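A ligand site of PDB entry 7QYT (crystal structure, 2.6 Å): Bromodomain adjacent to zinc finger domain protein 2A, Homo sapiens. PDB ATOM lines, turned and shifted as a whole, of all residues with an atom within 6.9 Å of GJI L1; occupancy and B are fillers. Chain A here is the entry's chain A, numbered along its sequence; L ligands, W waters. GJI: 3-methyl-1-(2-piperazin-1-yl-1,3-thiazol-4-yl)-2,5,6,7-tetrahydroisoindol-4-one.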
ATOM      1  N   TRP A  23      -1.760  -9.510 -16.204  1.00  0.00           N
ATOM      2  CA  TRP A  23      -0.408  -9.562 -15.651  1.00  0.00           C
ATOM      3  C   TRP A  23      -0.150  -8.569 -14.524  1.00  0.00           C
ATOM      4  O   TRP A  23       0.626  -8.938 -13.611  1.00  0.00           O
ATOM      5  CB  TRP A  23       0.617  -9.393 -16.786  1.00  0.00           C
ATOM      6  CG  TRP A  23       0.510  -8.117 -17.559  1.00  0.00           C
ATOM      7  CD1 TRP A  23      -0.228  -7.908 -18.686  1.00  0.00           C
ATOM      8  CD2 TRP A  23       1.158  -6.875 -17.259  1.00  0.00           C
ATOM      9  NE1 TRP A  23      -0.080  -6.608 -19.107  1.00  0.00           N
ATOM     10  CE2 TRP A  23       0.766  -5.950 -18.238  1.00  0.00           C
ATOM     11  CE3 TRP A  23       2.019  -6.445 -16.241  1.00  0.00           C
ATOM     12  CZ2 TRP A  23       1.217  -4.631 -18.248  1.00  0.00           C
ATOM     13  CZ3 TRP A  23       2.465  -5.134 -16.246  1.00  0.00           C
ATOM     14  CH2 TRP A  23       2.059  -4.246 -17.252  1.00  0.00           C
ATOM     15  N   PRO A  24      -0.702  -7.354 -14.478  1.00  0.00           N
ATOM     16  CA  PRO A  24      -0.392  -6.475 -13.341  1.00  0.00           C
ATOM     17  C   PRO A  24      -1.044  -6.897 -12.037  1.00  0.00           C
ATOM     18  O   PRO A  24      -0.701  -6.327 -10.992  1.00  0.00           O
ATOM     19  CB  PRO A  24      -0.921  -5.096 -13.784  1.00  0.00           C
ATOM     20  CG  PRO A  24      -1.192  -5.233 -15.244  1.00  0.00           C
ATOM     21  CD  PRO A  24      -1.565  -6.652 -15.442  1.00  0.00           C
ATOM     22  N   PHE A  25      -1.940  -7.884 -12.054  1.00  0.00           N
ATOM     23  CA  PHE A  25      -2.768  -8.188 -10.897  1.00  0.00           C
ATOM     24  C   PHE A  25      -2.645  -9.637 -10.439  1.00  0.00           C
ATOM     25  O   PHE A  25      -3.404 -10.050  -9.552  1.00  0.00           O
ATOM     26  CB  PHE A  25      -4.220  -7.850 -11.220  1.00  0.00           C
ATOM     27  CG  PHE A  25      -4.380  -6.563 -11.969  1.00  0.00           C
ATOM     28  CD1 PHE A  25      -4.182  -5.347 -11.330  1.00  0.00           C
ATOM     29  CD2 PHE A  25      -4.708  -6.565 -13.313  1.00  0.00           C
ATOM     30  CE1 PHE A  25      -4.316  -4.159 -12.014  1.00  0.00           C
ATOM     31  CE2 PHE A  25      -4.837  -5.370 -14.002  1.00  0.00           C
ATOM     32  CZ  PHE A  25      -4.645  -4.165 -13.344  1.00  0.00           C
ATOM     33  N   LEU A  26      -1.673 -10.358 -10.950  1.00  0.00           N
ATOM     34  CA  LEU A  26      -1.564 -11.781 -10.588  1.00  0.00           C
ATOM     35  C   LEU A  26      -0.914 -11.913  -9.216  1.00  0.00           C
ATOM     36  O   LEU A  26      -1.261 -12.823  -8.513  1.00  0.00           O
ATOM     37  CB  LEU A  26      -0.759 -12.455 -11.684  1.00  0.00           C
ATOM     38  CG  LEU A  26      -1.549 -12.701 -12.953  1.00  0.00           C
ATOM     39  CD1 LEU A  26      -0.688 -13.281 -14.039  1.00  0.00           C
ATOM     40  CD2 LEU A  26      -2.713 -13.601 -12.670  1.00  0.00           C
ATOM     41  N   GLU A  27       0.002 -11.006  -8.889  1.00  0.00           N
ATOM     42  CA  GLU A  27       0.716 -11.045  -7.582  1.00  0.00           C
ATOM     43  C   GLU A  27       0.581  -9.685  -6.886  1.00  0.00           C
ATOM     44  O   GLU A  27       0.427  -8.668  -7.596  1.00  0.00           O
ATOM     45  CB  GLU A  27       2.176 -11.413  -7.781  1.00  0.00           C
ATOM     46  CG  GLU A  27       2.393 -12.528  -8.789  1.00  0.00           C
ATOM     47  CD  GLU A  27       3.855 -12.879  -9.042  1.00  0.00           C
ATOM     48  OE1 GLU A  27       4.184 -13.198 -10.205  1.00  0.00           O
ATOM     49  OE2 GLU A  27       4.648 -12.837  -8.085  1.00  0.00           O
ATOM     50  N   PRO A  28       0.629  -9.621  -5.532  1.00  0.00           N
ATOM     51  CA  PRO A  28       0.517  -8.353  -4.806  1.00  0.00           C
ATOM     52  C   PRO A  28       1.629  -7.377  -5.193  1.00  0.00           C
ATOM     53  O   PRO A  28       2.743  -7.813  -5.412  1.00  0.00           O
ATOM     54  CB  PRO A  28       0.680  -8.765  -3.334  1.00  0.00           C
ATOM     55  CG  PRO A  28       0.311 -10.227  -3.308  1.00  0.00           C
ATOM     56  CD  PRO A  28       0.781 -10.772  -4.635  1.00  0.00           C
ATOM     57  N   VAL A  29       1.299  -6.085  -5.277  1.00  0.00           N
ATOM     58  CA  VAL A  29       2.297  -5.028  -5.642  1.00  0.00           C
ATOM     59  C   VAL A  29       3.369  -4.965  -4.556  1.00  0.00           C
ATOM     60  O   VAL A  29       3.007  -4.781  -3.379  1.00  0.00           O
ATOM     61  CB  VAL A  29       1.615  -3.660  -5.849  1.00  0.00           C
ATOM     62  CG1 VAL A  29       2.620  -2.519  -5.822  1.00  0.00           C
ATOM     63  CG2 VAL A  29       0.790  -3.619  -7.123  1.00  0.00           C
ATOM     64  N   VAL A  34       7.936   0.059  -5.766  1.00  0.00           N
ATOM     65  CA  VAL A  34       7.068   1.092  -6.319  1.00  0.00           C
ATOM     66  C   VAL A  34       7.075   2.256  -5.339  1.00  0.00           C
ATOM     67  O   VAL A  34       6.444   2.189  -4.268  1.00  0.00           O
ATOM     68  CB  VAL A  34       5.640   0.578  -6.553  1.00  0.00           C
ATOM     69  CG1 VAL A  34       4.781   1.682  -7.156  1.00  0.00           C
ATOM     70  CG2 VAL A  34       5.660  -0.638  -7.459  1.00  0.00           C
ATOM     71  N   TYR A  37       3.633   3.714  -3.290  1.00  0.00           N
ATOM     72  CA  TYR A  37       2.455   2.849  -3.293  1.00  0.00           C
ATOM     73  C   TYR A  37       1.863   2.718  -1.893  1.00  0.00           C
ATOM     74  O   TYR A  37       0.651   2.894  -1.701  1.00  0.00           O
ATOM     75  CB  TYR A  37       2.794   1.473  -3.868  1.00  0.00           C
ATOM     76  CG  TYR A  37       1.571   0.715  -4.329  1.00  0.00           C
ATOM     77  CD1 TYR A  37       0.955   1.025  -5.531  1.00  0.00           C
ATOM     78  CD2 TYR A  37       1.030  -0.302  -3.548  1.00  0.00           C
ATOM     79  CE1 TYR A  37      -0.169   0.339  -5.950  1.00  0.00           C
ATOM     80  CE2 TYR A  37      -0.099  -0.995  -3.963  1.00  0.00           C
ATOM     81  CZ  TYR A  37      -0.692  -0.674  -5.167  1.00  0.00           C
ATOM     82  OH  TYR A  37      -1.811  -1.353  -5.592  1.00  0.00           O
ATOM     83  N   ILE A  41      -2.091   3.848  -1.619  1.00  0.00           N
ATOM     84  CA  ILE A  41      -3.068   2.772  -1.706  1.00  0.00           C
ATOM     85  C   ILE A  41      -3.227   2.181  -0.312  1.00  0.00           C
ATOM     86  O   ILE A  41      -2.370   1.438   0.163  1.00  0.00           O
ATOM     87  CB  ILE A  41      -2.672   1.720  -2.746  1.00  0.00           C
ATOM     88  CG1 ILE A  41      -2.725   2.331  -4.142  1.00  0.00           C
ATOM     89  CG2 ILE A  41      -3.591   0.504  -2.653  1.00  0.00           C
ATOM     90  CD1 ILE A  41      -4.095   2.804  -4.552  1.00  0.00           C
ATOM     91  N   MET A  45      -5.045  -4.930  -3.098  1.00  0.00           N
ATOM     92  CA  MET A  45      -5.794  -6.124  -3.430  1.00  0.00           C
ATOM     93  C   MET A  45      -5.336  -6.627  -4.788  1.00  0.00           C
ATOM     94  O   MET A  45      -4.971  -5.833  -5.663  1.00  0.00           O
ATOM     95  CB  MET A  45      -7.308  -5.851  -3.442  1.00  0.00           C
ATOM     96  CG  MET A  45      -8.181  -7.088  -3.636  1.00  0.00           C
ATOM     97  SD  MET A  45      -7.738  -8.485  -2.600  1.00  0.00           S
ATOM     98  CE  MET A  45      -7.985  -7.799  -0.966  1.00  0.00           C
ATOM     99  N   VAL A  72      -9.383  -3.934  -6.742  1.00  0.00           N
ATOM    100  CA  VAL A  72      -8.196  -4.066  -7.582  1.00  0.00           C
ATOM    101  C   VAL A  72      -8.138  -2.945  -8.615  1.00  0.00           C
ATOM    102  O   VAL A  72      -7.072  -2.357  -8.861  1.00  0.00           O
ATOM    103  CB  VAL A  72      -8.183  -5.445  -8.266  1.00  0.00           C
ATOM    104  CG1 VAL A  72      -6.905  -5.605  -9.074  1.00  0.00           C
ATOM    105  CG2 VAL A  72      -8.319  -6.561  -7.241  1.00  0.00           C
ATOM    106  N   ASN A  75      -7.953   0.769  -6.952  1.00  0.00           N
ATOM    107  CA  ASN A  75      -6.528   0.952  -6.714  1.00  0.00           C
ATOM    108  C   ASN A  75      -5.796   1.320  -7.995  1.00  0.00           C
ATOM    109  O   ASN A  75      -5.023   2.276  -8.044  1.00  0.00           O
ATOM    110  CB  ASN A  75      -5.911  -0.318  -6.128  1.00  0.00           C
ATOM    111  CG  ASN A  75      -6.204  -0.497  -4.657  1.00  0.00           C
ATOM    112  OD1 ASN A  75      -6.887   0.311  -4.034  1.00  0.00           O
ATOM    113  ND2 ASN A  75      -5.660  -1.554  -4.080  1.00  0.00           N
ATOM    114  N   CYS A  76      -6.033   0.532  -9.048  1.00  0.00           N
ATOM    115  CA  CYS A  76      -5.300   0.709 -10.302  1.00  0.00           C
ATOM    116  C   CYS A  76      -5.516   2.099 -10.879  1.00  0.00           C
ATOM    117  O   CYS A  76      -4.559   2.744 -11.334  1.00  0.00           O
ATOM    118  CB  CYS A  76      -5.751  -0.358 -11.304  1.00  0.00           C
ATOM    119  SG  CYS A  76      -4.837  -0.311 -12.847  1.00  0.00           S
ATOM    120  N   PHE A  79      -3.711   4.917  -8.599  1.00  0.00           N
ATOM    121  CA  PHE A  79      -2.256   5.046  -8.652  1.00  0.00           C
ATOM    122  C   PHE A  79      -1.700   5.213 -10.058  1.00  0.00           C
ATOM    123  O   PHE A  79      -0.678   5.885 -10.227  1.00  0.00           O
ATOM    124  CB  PHE A  79      -1.591   3.828  -8.003  1.00  0.00           C
ATOM    125  CG  PHE A  79      -0.139   4.028  -7.714  1.00  0.00           C
ATOM    126  CD1 PHE A  79       0.267   4.580  -6.509  1.00  0.00           C
ATOM    127  CD2 PHE A  79       0.821   3.659  -8.639  1.00  0.00           C
ATOM    128  CE1 PHE A  79       1.606   4.763  -6.237  1.00  0.00           C
ATOM    129  CE2 PHE A  79       2.160   3.841  -8.368  1.00  0.00           C
ATOM    130  CZ  PHE A  79       2.555   4.397  -7.169  1.00  0.00           C
ATOM    131  N   ASN A  80      -2.340   4.633 -11.072  1.00  0.00           N
ATOM    132  CA  ASN A  80      -1.794   4.620 -12.425  1.00  0.00           C
ATOM    133  C   ASN A  80      -2.587   5.530 -13.342  1.00  0.00           C
ATOM    134  O   ASN A  80      -3.819   5.578 -13.275  1.00  0.00           O
ATOM    135  CB  ASN A  80      -1.773   3.201 -12.995  1.00  0.00           C
ATOM    136  CG  ASN A  80      -0.862   2.284 -12.233  1.00  0.00           C
ATOM    137  OD1 ASN A  80       0.342   2.251 -12.467  1.00  0.00           O
ATOM    138  ND2 ASN A  80      -1.435   1.542 -11.289  1.00  0.00           N
ATOM    139  N   VAL A  86       0.107  -0.257 -17.073  1.00  0.00           N
ATOM    140  CA  VAL A  86      -0.730  -0.875 -16.055  1.00  0.00           C
ATOM    141  C   VAL A  86      -2.148  -0.323 -16.114  1.00  0.00           C
ATOM    142  O   VAL A  86      -3.122  -1.071 -16.027  1.00  0.00           O
ATOM    143  CB  VAL A  86      -0.108  -0.689 -14.655  1.00  0.00           C
ATOM    144  CG1 VAL A  86      -1.160  -0.904 -13.573  1.00  0.00           C
ATOM    145  CG2 VAL A  86       1.069  -1.637 -14.458  1.00  0.00           C
HETATM  146  C11 GJI L   1       3.801  -8.488 -12.263  1.00  0.00           C
HETATM  147  C12 GJI L   1       4.768  -9.216 -11.333  1.00  0.00           C
HETATM  148  C14 GJI L   1       6.019  -9.540 -13.437  1.00  0.00           C
HETATM  149  C15 GJI L   1       5.637  -8.094 -13.898  1.00  0.00           C
HETATM  150  C01 GJI L   1      -1.290  -3.245 -10.045  1.00  0.00           C
HETATM  151  C02 GJI L   1       0.197  -2.983 -10.501  1.00  0.00           C
HETATM  152  C04 GJI L   1       2.204  -3.372 -11.416  1.00  0.00           C
HETATM  153  C05 GJI L   1       3.269  -4.105 -12.112  1.00  0.00           C
HETATM  154  C06 GJI L   1       4.379  -3.581 -12.832  1.00  0.00           C
HETATM  155  C08 GJI L   1       4.346  -6.032 -12.883  1.00  0.00           C
HETATM  156  C16 GJI L   1       2.235  -2.062 -10.909  1.00  0.00           C
HETATM  157  C17 GJI L   1       3.324  -0.950 -10.880  1.00  0.00           C
HETATM  158  C18 GJI L   1       2.690   0.474 -10.755  1.00  0.00           C
HETATM  159  C19 GJI L   1       1.691   0.558  -9.634  1.00  0.00           C
HETATM  160  C20 GJI L   1       0.646  -0.469  -9.678  1.00  0.00           C
HETATM  161  C22 GJI L   1       0.953  -1.826 -10.336  1.00  0.00           C
HETATM  162  N03 GJI L   1       0.994  -3.896 -11.161  1.00  0.00           N
HETATM  163  N09 GJI L   1       3.274  -5.566 -12.154  1.00  0.00           N
HETATM  164  N10 GJI L   1       4.601  -7.467 -13.041  1.00  0.00           N
HETATM  165  N13 GJI L   1       5.793  -9.911 -12.056  1.00  0.00           N
HETATM  166  O21 GJI L   1      -0.442  -0.258  -9.210  1.00  0.00           O
HETATM  167  S07 GJI L   1       5.243  -4.797 -13.417  1.00  0.00           S
HETATM  168  C11 GJI L   2      11.447  -3.953 -13.437  1.00  0.00           C
HETATM  169  C12 GJI L   2      12.568  -2.967 -13.820  1.00  0.00           C
HETATM  170  C14 GJI L   2      13.877  -4.639 -14.819  1.00  0.00           C
HETATM  171  C15 GJI L   2      12.869  -5.773 -14.495  1.00  0.00           C
HETATM  172  C01 GJI L   2       5.723  -8.526  -7.862  1.00  0.00           C
HETATM  173  C02 GJI L   2       6.705  -7.664  -8.766  1.00  0.00           C
HETATM  174  C04 GJI L   2       8.396  -7.151 -10.152  1.00  0.00           C
HETATM  175  C05 GJI L   2       9.589  -7.232 -11.034  1.00  0.00           C
HETATM  176  C06 GJI L   2      10.432  -8.355 -11.263  1.00  0.00           C
HETATM  177  C08 GJI L   2      11.185  -6.412 -12.577  1.00  0.00           C
HETATM  178  C16 GJI L   2       7.698  -5.958  -9.858  1.00  0.00           C
HETATM  179  C17 GJI L   2       7.889  -4.465 -10.282  1.00  0.00           C
HETATM  180  C18 GJI L   2       6.530  -3.697 -10.314  1.00  0.00           C
HETATM  181  C19 GJI L   2       5.723  -3.834  -9.057  1.00  0.00           C
HETATM  182  C20 GJI L   2       5.681  -5.182  -8.476  1.00  0.00           C
HETATM  183  C22 GJI L   2       6.627  -6.291  -8.986  1.00  0.00           C
HETATM  184  N03 GJI L   2       7.783  -8.157  -9.489  1.00  0.00           N
HETATM  185  N09 GJI L   2      10.045  -6.093 -11.824  1.00  0.00           N
HETATM  186  N10 GJI L   2      11.827  -5.432 -13.471  1.00  0.00           N
HETATM  187  N13 GJI L   2      13.253  -3.369 -14.989  1.00  0.00           N
HETATM  188  O21 GJI L   2       4.902  -5.419  -7.577  1.00  0.00           O
HETATM  189  S07 GJI L   2      11.583  -7.957 -12.304  1.00  0.00           S
HETATM  190  O   HOH W   1      -4.380  -2.475  -8.697  1.00  0.00           O
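ND2 of Asn 80 sits close to O of Cys 76 (3.3 Å).
The side-chain sulfur (SG) of Cys 76 is in hydrogen-bond range of the backbone carbonyl oxygen (O) of Val 86 (3.7 Å).
ND2 of Asn 80 sits at hydrogen-bond distance from O21 of GJI L1.
The backbone carbonyl oxygen of Pro 24 lies within hydrogen-bond range of a nitrogen (N03) of GJI L1 (3.0 Å).
Residues that only touch GJI L1: Trp 23 (3.5 Å), Phe 25 (3.7 Å), Val 29 (3.5 Å), Tyr 37 (3.3 Å), Phe 79 (3.4 Å) and Val 86 (3.7 Å).
Hydrophobic or aromatic side chains that line GJI L1: Trp 23, Pro 24, Phe 25, Val 29, Tyr 37, Phe 79 and Val 86.
Eight residues have an atom within 4 Å of GJI L1: Trp 23, Pro 24, Phe 25, Val 29, Tyr 37, Phe 79, Asn 80 and Val 86.
The nearest printed residue that does not touch GJI L1 is Glu 27 (4.1 Å).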
